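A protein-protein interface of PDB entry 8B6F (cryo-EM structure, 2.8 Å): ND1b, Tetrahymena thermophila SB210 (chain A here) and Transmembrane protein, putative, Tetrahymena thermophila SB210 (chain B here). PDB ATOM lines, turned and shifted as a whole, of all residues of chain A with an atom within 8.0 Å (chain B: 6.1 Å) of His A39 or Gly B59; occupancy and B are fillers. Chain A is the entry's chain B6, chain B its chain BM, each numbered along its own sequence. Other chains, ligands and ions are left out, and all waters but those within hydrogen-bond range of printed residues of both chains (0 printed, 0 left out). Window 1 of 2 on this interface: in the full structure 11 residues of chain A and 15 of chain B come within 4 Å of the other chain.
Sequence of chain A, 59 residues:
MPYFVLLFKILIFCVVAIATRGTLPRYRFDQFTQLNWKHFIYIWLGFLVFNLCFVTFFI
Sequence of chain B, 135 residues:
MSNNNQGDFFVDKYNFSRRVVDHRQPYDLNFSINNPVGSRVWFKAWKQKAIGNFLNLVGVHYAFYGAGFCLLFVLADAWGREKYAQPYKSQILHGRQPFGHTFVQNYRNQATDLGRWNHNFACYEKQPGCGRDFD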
ATOM      1  N   PHE A  32      14.571  27.171  40.606  1.00  0.00           N
ATOM      2  CA  PHE A  32      13.908  27.447  39.338  1.00  0.00           C
ATOM      3  C   PHE A  32      14.694  28.451  38.510  1.00  0.00           C
ATOM      4  O   PHE A  32      14.778  28.324  37.284  1.00  0.00           O
ATOM      5  CB  PHE A  32      12.491  27.959  39.567  1.00  0.00           C
ATOM      6  CG  PHE A  32      11.841  28.463  38.319  1.00  0.00           C
ATOM      7  CD1 PHE A  32      11.593  27.606  37.261  1.00  0.00           C
ATOM      8  CD2 PHE A  32      11.505  29.798  38.188  1.00  0.00           C
ATOM      9  CE1 PHE A  32      11.007  28.068  36.102  1.00  0.00           C
ATOM     10  CE2 PHE A  32      10.920  30.267  37.032  1.00  0.00           C
ATOM     11  CZ  PHE A  32      10.670  29.400  35.987  1.00  0.00           C
ATOM     12  N   THR A  33      15.267  29.462  39.159  1.00  0.00           N
ATOM     13  CA  THR A  33      16.047  30.443  38.421  1.00  0.00           C
ATOM     14  C   THR A  33      17.258  29.797  37.766  1.00  0.00           C
ATOM     15  O   THR A  33      17.558  30.065  36.598  1.00  0.00           O
ATOM     16  CB  THR A  33      16.477  31.567  39.355  1.00  0.00           C
ATOM     17  OG1 THR A  33      15.344  32.050  40.086  1.00  0.00           O
ATOM     18  CG2 THR A  33      17.062  32.696  38.567  1.00  0.00           C
ATOM     19  N   GLN A  34      17.964  28.939  38.501  1.00  0.00           N
ATOM     20  CA  GLN A  34      19.101  28.239  37.915  1.00  0.00           C
ATOM     21  C   GLN A  34      18.652  27.374  36.745  1.00  0.00           C
ATOM     22  O   GLN A  34      19.249  27.410  35.664  1.00  0.00           O
ATOM     23  CB  GLN A  34      19.805  27.396  38.977  1.00  0.00           C
ATOM     24  CG  GLN A  34      20.492  28.222  40.046  1.00  0.00           C
ATOM     25  CD  GLN A  34      21.083  27.368  41.145  1.00  0.00           C
ATOM     26  OE1 GLN A  34      21.038  26.141  41.085  1.00  0.00           O
ATOM     27  NE2 GLN A  34      21.646  28.016  42.158  1.00  0.00           N
ATOM     28  N   LEU A  35      17.596  26.582  36.945  1.00  0.00           N
ATOM     29  CA  LEU A  35      17.086  25.752  35.861  1.00  0.00           C
ATOM     30  C   LEU A  35      16.780  26.599  34.636  1.00  0.00           C
ATOM     31  O   LEU A  35      17.219  26.290  33.523  1.00  0.00           O
ATOM     32  CB  LEU A  35      15.830  25.008  36.315  1.00  0.00           C
ATOM     33  CG  LEU A  35      16.008  23.901  37.352  1.00  0.00           C
ATOM     34  CD1 LEU A  35      14.660  23.361  37.791  1.00  0.00           C
ATOM     35  CD2 LEU A  35      16.874  22.779  36.798  1.00  0.00           C
ATOM     36  N   ASN A  36      16.019  27.676  34.826  1.00  0.00           N
ATOM     37  CA  ASN A  36      15.650  28.531  33.707  1.00  0.00           C
ATOM     38  C   ASN A  36      16.891  29.038  32.979  1.00  0.00           C
ATOM     39  O   ASN A  36      17.116  28.722  31.806  1.00  0.00           O
ATOM     40  CB  ASN A  36      14.793  29.690  34.218  1.00  0.00           C
ATOM     41  CG  ASN A  36      14.240  30.546  33.104  1.00  0.00           C
ATOM     42  OD1 ASN A  36      14.373  30.219  31.927  1.00  0.00           O
ATOM     43  ND2 ASN A  36      13.583  31.637  33.473  1.00  0.00           N
ATOM     44  N   TRP A  37      17.708  29.837  33.667  1.00  0.00           N
ATOM     45  CA  TRP A  37      18.814  30.528  33.020  1.00  0.00           C
ATOM     46  C   TRP A  37      19.924  29.597  32.547  1.00  0.00           C
ATOM     47  O   TRP A  37      20.797  30.047  31.800  1.00  0.00           O
ATOM     48  CB  TRP A  37      19.401  31.567  33.975  1.00  0.00           C
ATOM     49  CG  TRP A  37      18.507  32.740  34.200  1.00  0.00           C
ATOM     50  CD1 TRP A  37      17.416  32.796  35.016  1.00  0.00           C
ATOM     51  CD2 TRP A  37      18.627  34.033  33.600  1.00  0.00           C
ATOM     52  NE1 TRP A  37      16.849  34.045  34.962  1.00  0.00           N
ATOM     53  CE2 TRP A  37      17.576  34.824  34.100  1.00  0.00           C
ATOM     54  CE3 TRP A  37      19.524  34.598  32.689  1.00  0.00           C
ATOM     55  CZ2 TRP A  37      17.394  36.150  33.716  1.00  0.00           C
ATOM     56  CZ3 TRP A  37      19.343  35.915  32.310  1.00  0.00           C
ATOM     57  CH2 TRP A  37      18.285  36.676  32.823  1.00  0.00           C
ATOM     58  N   LYS A  38      19.922  28.327  32.954  1.00  0.00           N
ATOM     59  CA  LYS A  38      20.946  27.391  32.502  1.00  0.00           C
ATOM     60  C   LYS A  38      20.466  26.431  31.426  1.00  0.00           C
ATOM     61  O   LYS A  38      21.278  25.988  30.608  1.00  0.00           O
ATOM     62  CB  LYS A  38      21.478  26.574  33.684  1.00  0.00           C
ATOM     63  CG  LYS A  38      22.198  27.403  34.734  1.00  0.00           C
ATOM     64  CD  LYS A  38      22.659  26.535  35.892  1.00  0.00           C
ATOM     65  CE  LYS A  38      23.275  27.371  37.001  1.00  0.00           C
ATOM     66  NZ  LYS A  38      24.490  28.100  36.548  1.00  0.00           N
ATOM     67  N   HIS A  39      19.179  26.091  31.403  1.00  0.00           N
ATOM     68  CA  HIS A  39      18.662  25.115  30.455  1.00  0.00           C
ATOM     69  C   HIS A  39      17.575  25.681  29.557  1.00  0.00           C
ATOM     70  O   HIS A  39      17.645  25.523  28.334  1.00  0.00           O
ATOM     71  CB  HIS A  39      18.125  23.895  31.226  1.00  0.00           C
ATOM     72  CG  HIS A  39      17.677  22.771  30.346  1.00  0.00           C
ATOM     73  ND1 HIS A  39      18.532  22.106  29.493  1.00  0.00           N
ATOM     74  CD2 HIS A  39      16.464  22.191  30.190  1.00  0.00           C
ATOM     75  CE1 HIS A  39      17.863  21.170  28.845  1.00  0.00           C
ATOM     76  NE2 HIS A  39      16.606  21.198  29.252  1.00  0.00           N
ATOM     77  N   PHE A  40      16.578  26.355  30.127  1.00  0.00           N
ATOM     78  CA  PHE A  40      15.365  26.655  29.375  1.00  0.00           C
ATOM     79  C   PHE A  40      15.553  27.808  28.402  1.00  0.00           C
ATOM     80  O   PHE A  40      14.926  27.821  27.340  1.00  0.00           O
ATOM     81  CB  PHE A  40      14.210  26.952  30.331  1.00  0.00           C
ATOM     82  CG  PHE A  40      13.760  25.759  31.126  1.00  0.00           C
ATOM     83  CD1 PHE A  40      13.668  24.510  30.532  1.00  0.00           C
ATOM     84  CD2 PHE A  40      13.436  25.883  32.464  1.00  0.00           C
ATOM     85  CE1 PHE A  40      13.257  23.412  31.256  1.00  0.00           C
ATOM     86  CE2 PHE A  40      13.024  24.786  33.195  1.00  0.00           C
ATOM     87  CZ  PHE A  40      12.935  23.549  32.590  1.00  0.00           C
ATOM     88  N   ILE A  41      16.409  28.775  28.734  1.00  0.00           N
ATOM     89  CA  ILE A  41      16.699  29.844  27.785  1.00  0.00           C
ATOM     90  C   ILE A  41      17.362  29.274  26.537  1.00  0.00           C
ATOM     91  O   ILE A  41      17.010  29.639  25.409  1.00  0.00           O
ATOM     92  CB  ILE A  41      17.557  30.936  28.455  1.00  0.00           C
ATOM     93  CG1 ILE A  41      17.730  32.127  27.510  1.00  0.00           C
ATOM     94  CG2 ILE A  41      18.917  30.388  28.874  1.00  0.00           C
ATOM     95  CD1 ILE A  41      18.326  33.353  28.166  1.00  0.00           C
ATOM     96  N   TYR A  42      18.323  28.368  26.718  1.00  0.00           N
ATOM     97  CA  TYR A  42      18.948  27.721  25.570  1.00  0.00           C
ATOM     98  C   TYR A  42      17.938  26.895  24.785  1.00  0.00           C
ATOM     99  O   TYR A  42      17.972  26.870  23.550  1.00  0.00           O
ATOM    100  CB  TYR A  42      20.107  26.841  26.034  1.00  0.00           C
ATOM    101  CG  TYR A  42      21.195  27.587  26.768  1.00  0.00           C
ATOM    102  CD1 TYR A  42      22.194  28.260  26.080  1.00  0.00           C
ATOM    103  CD2 TYR A  42      21.227  27.604  28.155  1.00  0.00           C
ATOM    104  CE1 TYR A  42      23.195  28.936  26.755  1.00  0.00           C
ATOM    105  CE2 TYR A  42      22.219  28.276  28.838  1.00  0.00           C
ATOM    106  CZ  TYR A  42      23.199  28.939  28.134  1.00  0.00           C
ATOM    107  OH  TYR A  42      24.186  29.607  28.820  1.00  0.00           O
ATOM    108  N   ILE A  43      17.037  26.201  25.483  1.00  0.00           N
ATOM    109  CA  ILE A  43      16.018  25.410  24.797  1.00  0.00           C
ATOM    110  C   ILE A  43      15.139  26.312  23.940  1.00  0.00           C
ATOM    111  O   ILE A  43      14.842  25.998  22.780  1.00  0.00           O
ATOM    112  CB  ILE A  43      15.184  24.610  25.816  1.00  0.00           C
ATOM    113  CG1 ILE A  43      16.033  23.515  26.472  1.00  0.00           C
ATOM    114  CG2 ILE A  43      13.942  24.012  25.152  1.00  0.00           C
ATOM    115  CD1 ILE A  43      16.383  22.349  25.571  1.00  0.00           C
ATOM    116  N   TRP A  44      14.700  27.442  24.498  1.00  0.00           N
ATOM    117  CA  TRP A  44      13.861  28.361  23.735  1.00  0.00           C
ATOM    118  C   TRP A  44      14.597  28.888  22.511  1.00  0.00           C
ATOM    119  O   TRP A  44      14.042  28.927  21.407  1.00  0.00           O
ATOM    120  CB  TRP A  44      13.416  29.525  24.617  1.00  0.00           C
ATOM    121  CG  TRP A  44      12.294  29.216  25.557  1.00  0.00           C
ATOM    122  CD1 TRP A  44      12.337  29.238  26.921  1.00  0.00           C
ATOM    123  CD2 TRP A  44      10.957  28.847  25.204  1.00  0.00           C
ATOM    124  NE1 TRP A  44      11.110  28.904  27.437  1.00  0.00           N
ATOM    125  CE2 TRP A  44      10.245  28.660  26.404  1.00  0.00           C
ATOM    126  CE3 TRP A  44      10.294  28.654  23.988  1.00  0.00           C
ATOM    127  CZ2 TRP A  44       8.903  28.289  26.424  1.00  0.00           C
ATOM    128  CZ3 TRP A  44       8.960  28.288  24.011  1.00  0.00           C
ATOM    129  CH2 TRP A  44       8.280  28.108  25.220  1.00  0.00           C
ATOM    130  N   LEU A  45      15.851  29.307  22.689  1.00  0.00           N
ATOM    131  CA  LEU A  45      16.606  29.859  21.570  1.00  0.00           C
ATOM    132  C   LEU A  45      16.859  28.805  20.503  1.00  0.00           C
ATOM    133  O   LEU A  45      16.736  29.084  19.307  1.00  0.00           O
ATOM    134  CB  LEU A  45      17.922  30.460  22.064  1.00  0.00           C
ATOM    135  CG  LEU A  45      17.781  31.712  22.936  1.00  0.00           C
ATOM    136  CD1 LEU A  45      19.124  32.127  23.505  1.00  0.00           C
ATOM    137  CD2 LEU A  45      17.165  32.863  22.155  1.00  0.00           C
ATOM    138  N   GLY A  46      17.188  27.581  20.914  1.00  0.00           N
ATOM    139  CA  GLY A  46      17.366  26.516  19.944  1.00  0.00           C
ATOM    140  C   GLY A  46      16.087  26.208  19.189  1.00  0.00           C
ATOM    141  O   GLY A  46      16.110  25.982  17.978  1.00  0.00           O
ATOM    142  N   PHE B  54      27.488  16.897  27.837  1.00  0.00           N
ATOM    143  CA  PHE B  54      26.062  16.918  27.529  1.00  0.00           C
ATOM    144  C   PHE B  54      25.227  16.813  28.796  1.00  0.00           C
ATOM    145  O   PHE B  54      24.219  17.513  28.942  1.00  0.00           O
ATOM    146  CB  PHE B  54      25.706  15.784  26.570  1.00  0.00           C
ATOM    147  CG  PHE B  54      24.276  15.812  26.118  1.00  0.00           C
ATOM    148  CD1 PHE B  54      23.283  15.212  26.873  1.00  0.00           C
ATOM    149  CD2 PHE B  54      23.925  16.447  24.941  1.00  0.00           C
ATOM    150  CE1 PHE B  54      21.966  15.245  26.460  1.00  0.00           C
ATOM    151  CE2 PHE B  54      22.611  16.484  24.523  1.00  0.00           C
ATOM    152  CZ  PHE B  54      21.630  15.882  25.284  1.00  0.00           C
ATOM    153  N   LEU B  57      25.323  20.197  30.430  1.00  0.00           N
ATOM    154  CA  LEU B  57      24.561  21.182  29.658  1.00  0.00           C
ATOM    155  C   LEU B  57      23.790  20.469  28.555  1.00  0.00           C
ATOM    156  O   LEU B  57      24.236  20.394  27.409  1.00  0.00           O
ATOM    157  CB  LEU B  57      25.490  22.237  29.084  1.00  0.00           C
ATOM    158  CG  LEU B  57      26.194  23.137  30.087  1.00  0.00           C
ATOM    159  CD1 LEU B  57      27.226  24.022  29.411  1.00  0.00           C
ATOM    160  CD2 LEU B  57      25.134  23.973  30.772  1.00  0.00           C
ATOM    161  N   VAL B  58      22.612  19.955  28.907  1.00  0.00           N
ATOM    162  CA  VAL B  58      21.709  19.418  27.896  1.00  0.00           C
ATOM    163  C   VAL B  58      21.203  20.534  26.991  1.00  0.00           C
ATOM    164  O   VAL B  58      21.191  20.404  25.761  1.00  0.00           O
ATOM    165  CB  VAL B  58      20.546  18.665  28.568  1.00  0.00           C
ATOM    166  CG1 VAL B  58      19.591  18.104  27.526  1.00  0.00           C
ATOM    167  CG2 VAL B  58      21.079  17.556  29.461  1.00  0.00           C
ATOM    168  N   GLY B  59      20.773  21.649  27.586  1.00  0.00           N
ATOM    169  CA  GLY B  59      20.193  22.722  26.795  1.00  0.00           C
ATOM    170  C   GLY B  59      21.192  23.386  25.869  1.00  0.00           C
ATOM    171  O   GLY B  59      20.883  23.673  24.710  1.00  0.00           O
ATOM    172  N   VAL B  60      22.403  23.649  26.368  1.00  0.00           N
ATOM    173  CA  VAL B  60      23.416  24.305  25.545  1.00  0.00           C
ATOM    174  C   VAL B  60      23.795  23.426  24.364  1.00  0.00           C
ATOM    175  O   VAL B  60      23.911  23.901  23.228  1.00  0.00           O
ATOM    176  CB  VAL B  60      24.647  24.669  26.394  1.00  0.00           C
ATOM    177  CG1 VAL B  60      25.642  25.467  25.573  1.00  0.00           C
ATOM    178  CG2 VAL B  60      24.231  25.452  27.629  1.00  0.00           C
ATOM    179  N   HIS B  61      23.999  22.131  24.610  1.00  0.00           N
ATOM    180  CA  HIS B  61      24.350  21.229  23.520  1.00  0.00           C
ATOM    181  C   HIS B  61      23.261  21.206  22.461  1.00  0.00           C
ATOM    182  O   HIS B  61      23.550  21.233  21.259  1.00  0.00           O
ATOM    183  CB  HIS B  61      24.606  19.825  24.061  1.00  0.00           C
ATOM    184  CG  HIS B  61      25.989  19.631  24.594  1.00  0.00           C
ATOM    185  ND1 HIS B  61      26.454  20.290  25.712  1.00  0.00           N
ATOM    186  CD2 HIS B  61      27.012  18.858  24.161  1.00  0.00           C
ATOM    187  CE1 HIS B  61      27.704  19.930  25.944  1.00  0.00           C
ATOM    188  NE2 HIS B  61      28.066  19.062  25.018  1.00  0.00           N
ATOM    189  N   TYR B  62      22.000  21.148  22.885  1.00  0.00           N
ATOM    190  CA  TYR B  62      20.898  21.260  21.937  1.00  0.00           C
ATOM    191  C   TYR B  62      21.020  22.543  21.125  1.00  0.00           C
ATOM    192  O   TYR B  62      21.176  22.511  19.900  1.00  0.00           O
ATOM    193  CB  TYR B  62      19.566  21.217  22.690  1.00  0.00           C
ATOM    194  CG  TYR B  62      18.372  21.594  21.849  1.00  0.00           C
ATOM    195  CD1 TYR B  62      17.905  20.745  20.856  1.00  0.00           C
ATOM    196  CD2 TYR B  62      17.707  22.792  22.054  1.00  0.00           C
ATOM    197  CE1 TYR B  62      16.812  21.082  20.086  1.00  0.00           C
ATOM    198  CE2 TYR B  62      16.611  23.138  21.289  1.00  0.00           C
ATOM    199  CZ  TYR B  62      16.169  22.278  20.307  1.00  0.00           C
ATOM    200  OH  TYR B  62      15.079  22.615  19.541  1.00  0.00           O
ATOM    201  N   ALA B  63      20.930  23.690  21.802  1.00  0.00           N
ATOM    202  CA  ALA B  63      20.858  24.967  21.102  1.00  0.00           C
ATOM    203  C   ALA B  63      22.025  25.172  20.145  1.00  0.00           C
ATOM    204  O   ALA B  63      21.873  25.850  19.125  1.00  0.00           O
ATOM    205  CB  ALA B  63      20.811  26.110  22.114  1.00  0.00           C
ATOM    206  N   PHE B  64      23.197  24.613  20.454  1.00  0.00           N
ATOM    207  CA  PHE B  64      24.369  24.812  19.606  1.00  0.00           C
ATOM    208  C   PHE B  64      24.480  23.756  18.510  1.00  0.00           C
ATOM    209  O   PHE B  64      24.468  24.084  17.320  1.00  0.00           O
ATOM    210  CB  PHE B  64      25.639  24.822  20.466  1.00  0.00           C
ATOM    211  CG  PHE B  64      25.934  26.155  21.095  1.00  0.00           C
ATOM    212  CD1 PHE B  64      25.367  26.506  22.307  1.00  0.00           C
ATOM    213  CD2 PHE B  64      26.776  27.057  20.469  1.00  0.00           C
ATOM    214  CE1 PHE B  64      25.636  27.729  22.886  1.00  0.00           C
ATOM    215  CE2 PHE B  64      27.049  28.282  21.042  1.00  0.00           C
ATOM    216  CZ  PHE B  64      26.477  28.619  22.252  1.00  0.00           C
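Hydrophobic or aromatic side chains of chain B within 4 Å of the printed part of chain A: Val B58, Val B60, Tyr B62 and Ala B63. Hydrophobic or aromatic side chains of chain A that line the printed part of chain B: His A39, Tyr A42 and Ile A43. Along chain A the printed residues that touch a printed residue of chain B span positions 39 to 46. Among the printed residues, 8 pairs touch across the chains.
His A39 touches two residues of chain B. Printed residues of chain A within 4 Å of Gly B59: His A39 and Tyr A42. Of the printed residues of chain A, Val B58 touches His A39 (3.7 Å). Printed residues of chain A within 4 Å of Ala B63: Tyr A42 and Gly A46. Of the printed residues of chain A, Val B60 touches Tyr A42 (3.7 Å). Printed residues of chain B within 4 Å of Tyr A42: Gly B59, Val B60 and Ala B63. Of the printed residues of chain B, Gly A46 touches Tyr B62 and Ala B63. Asn A36 touches none of the printed residues of chain B. His B61 touches none of the printed residues of chain A. The nearest printed residue of chain A that does not touch Gly B59 is Ile A43 (4.02 Å).
CE1 of His A39 touches CB of Val B58, 3.7 Å away. O of Gly B59 touches CB of Tyr A42, 3.5 Å away. Tyr A42 touches Val B60 (CZ to CG2, 3.7 Å). Tyr A42 touches Ala B63. Ile A43 touches Tyr B62. Gly A46 touches Tyr B62 (CA to CE2, 3.7 Å). Ala B63 touches Gly A46 (CA to CA, 3.99 Å).
A ring nitrogen (ND1) of His A39 sits at hydrogen-bond distance from the backbone NH (N) of Gly B59, at 3.0 Å.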
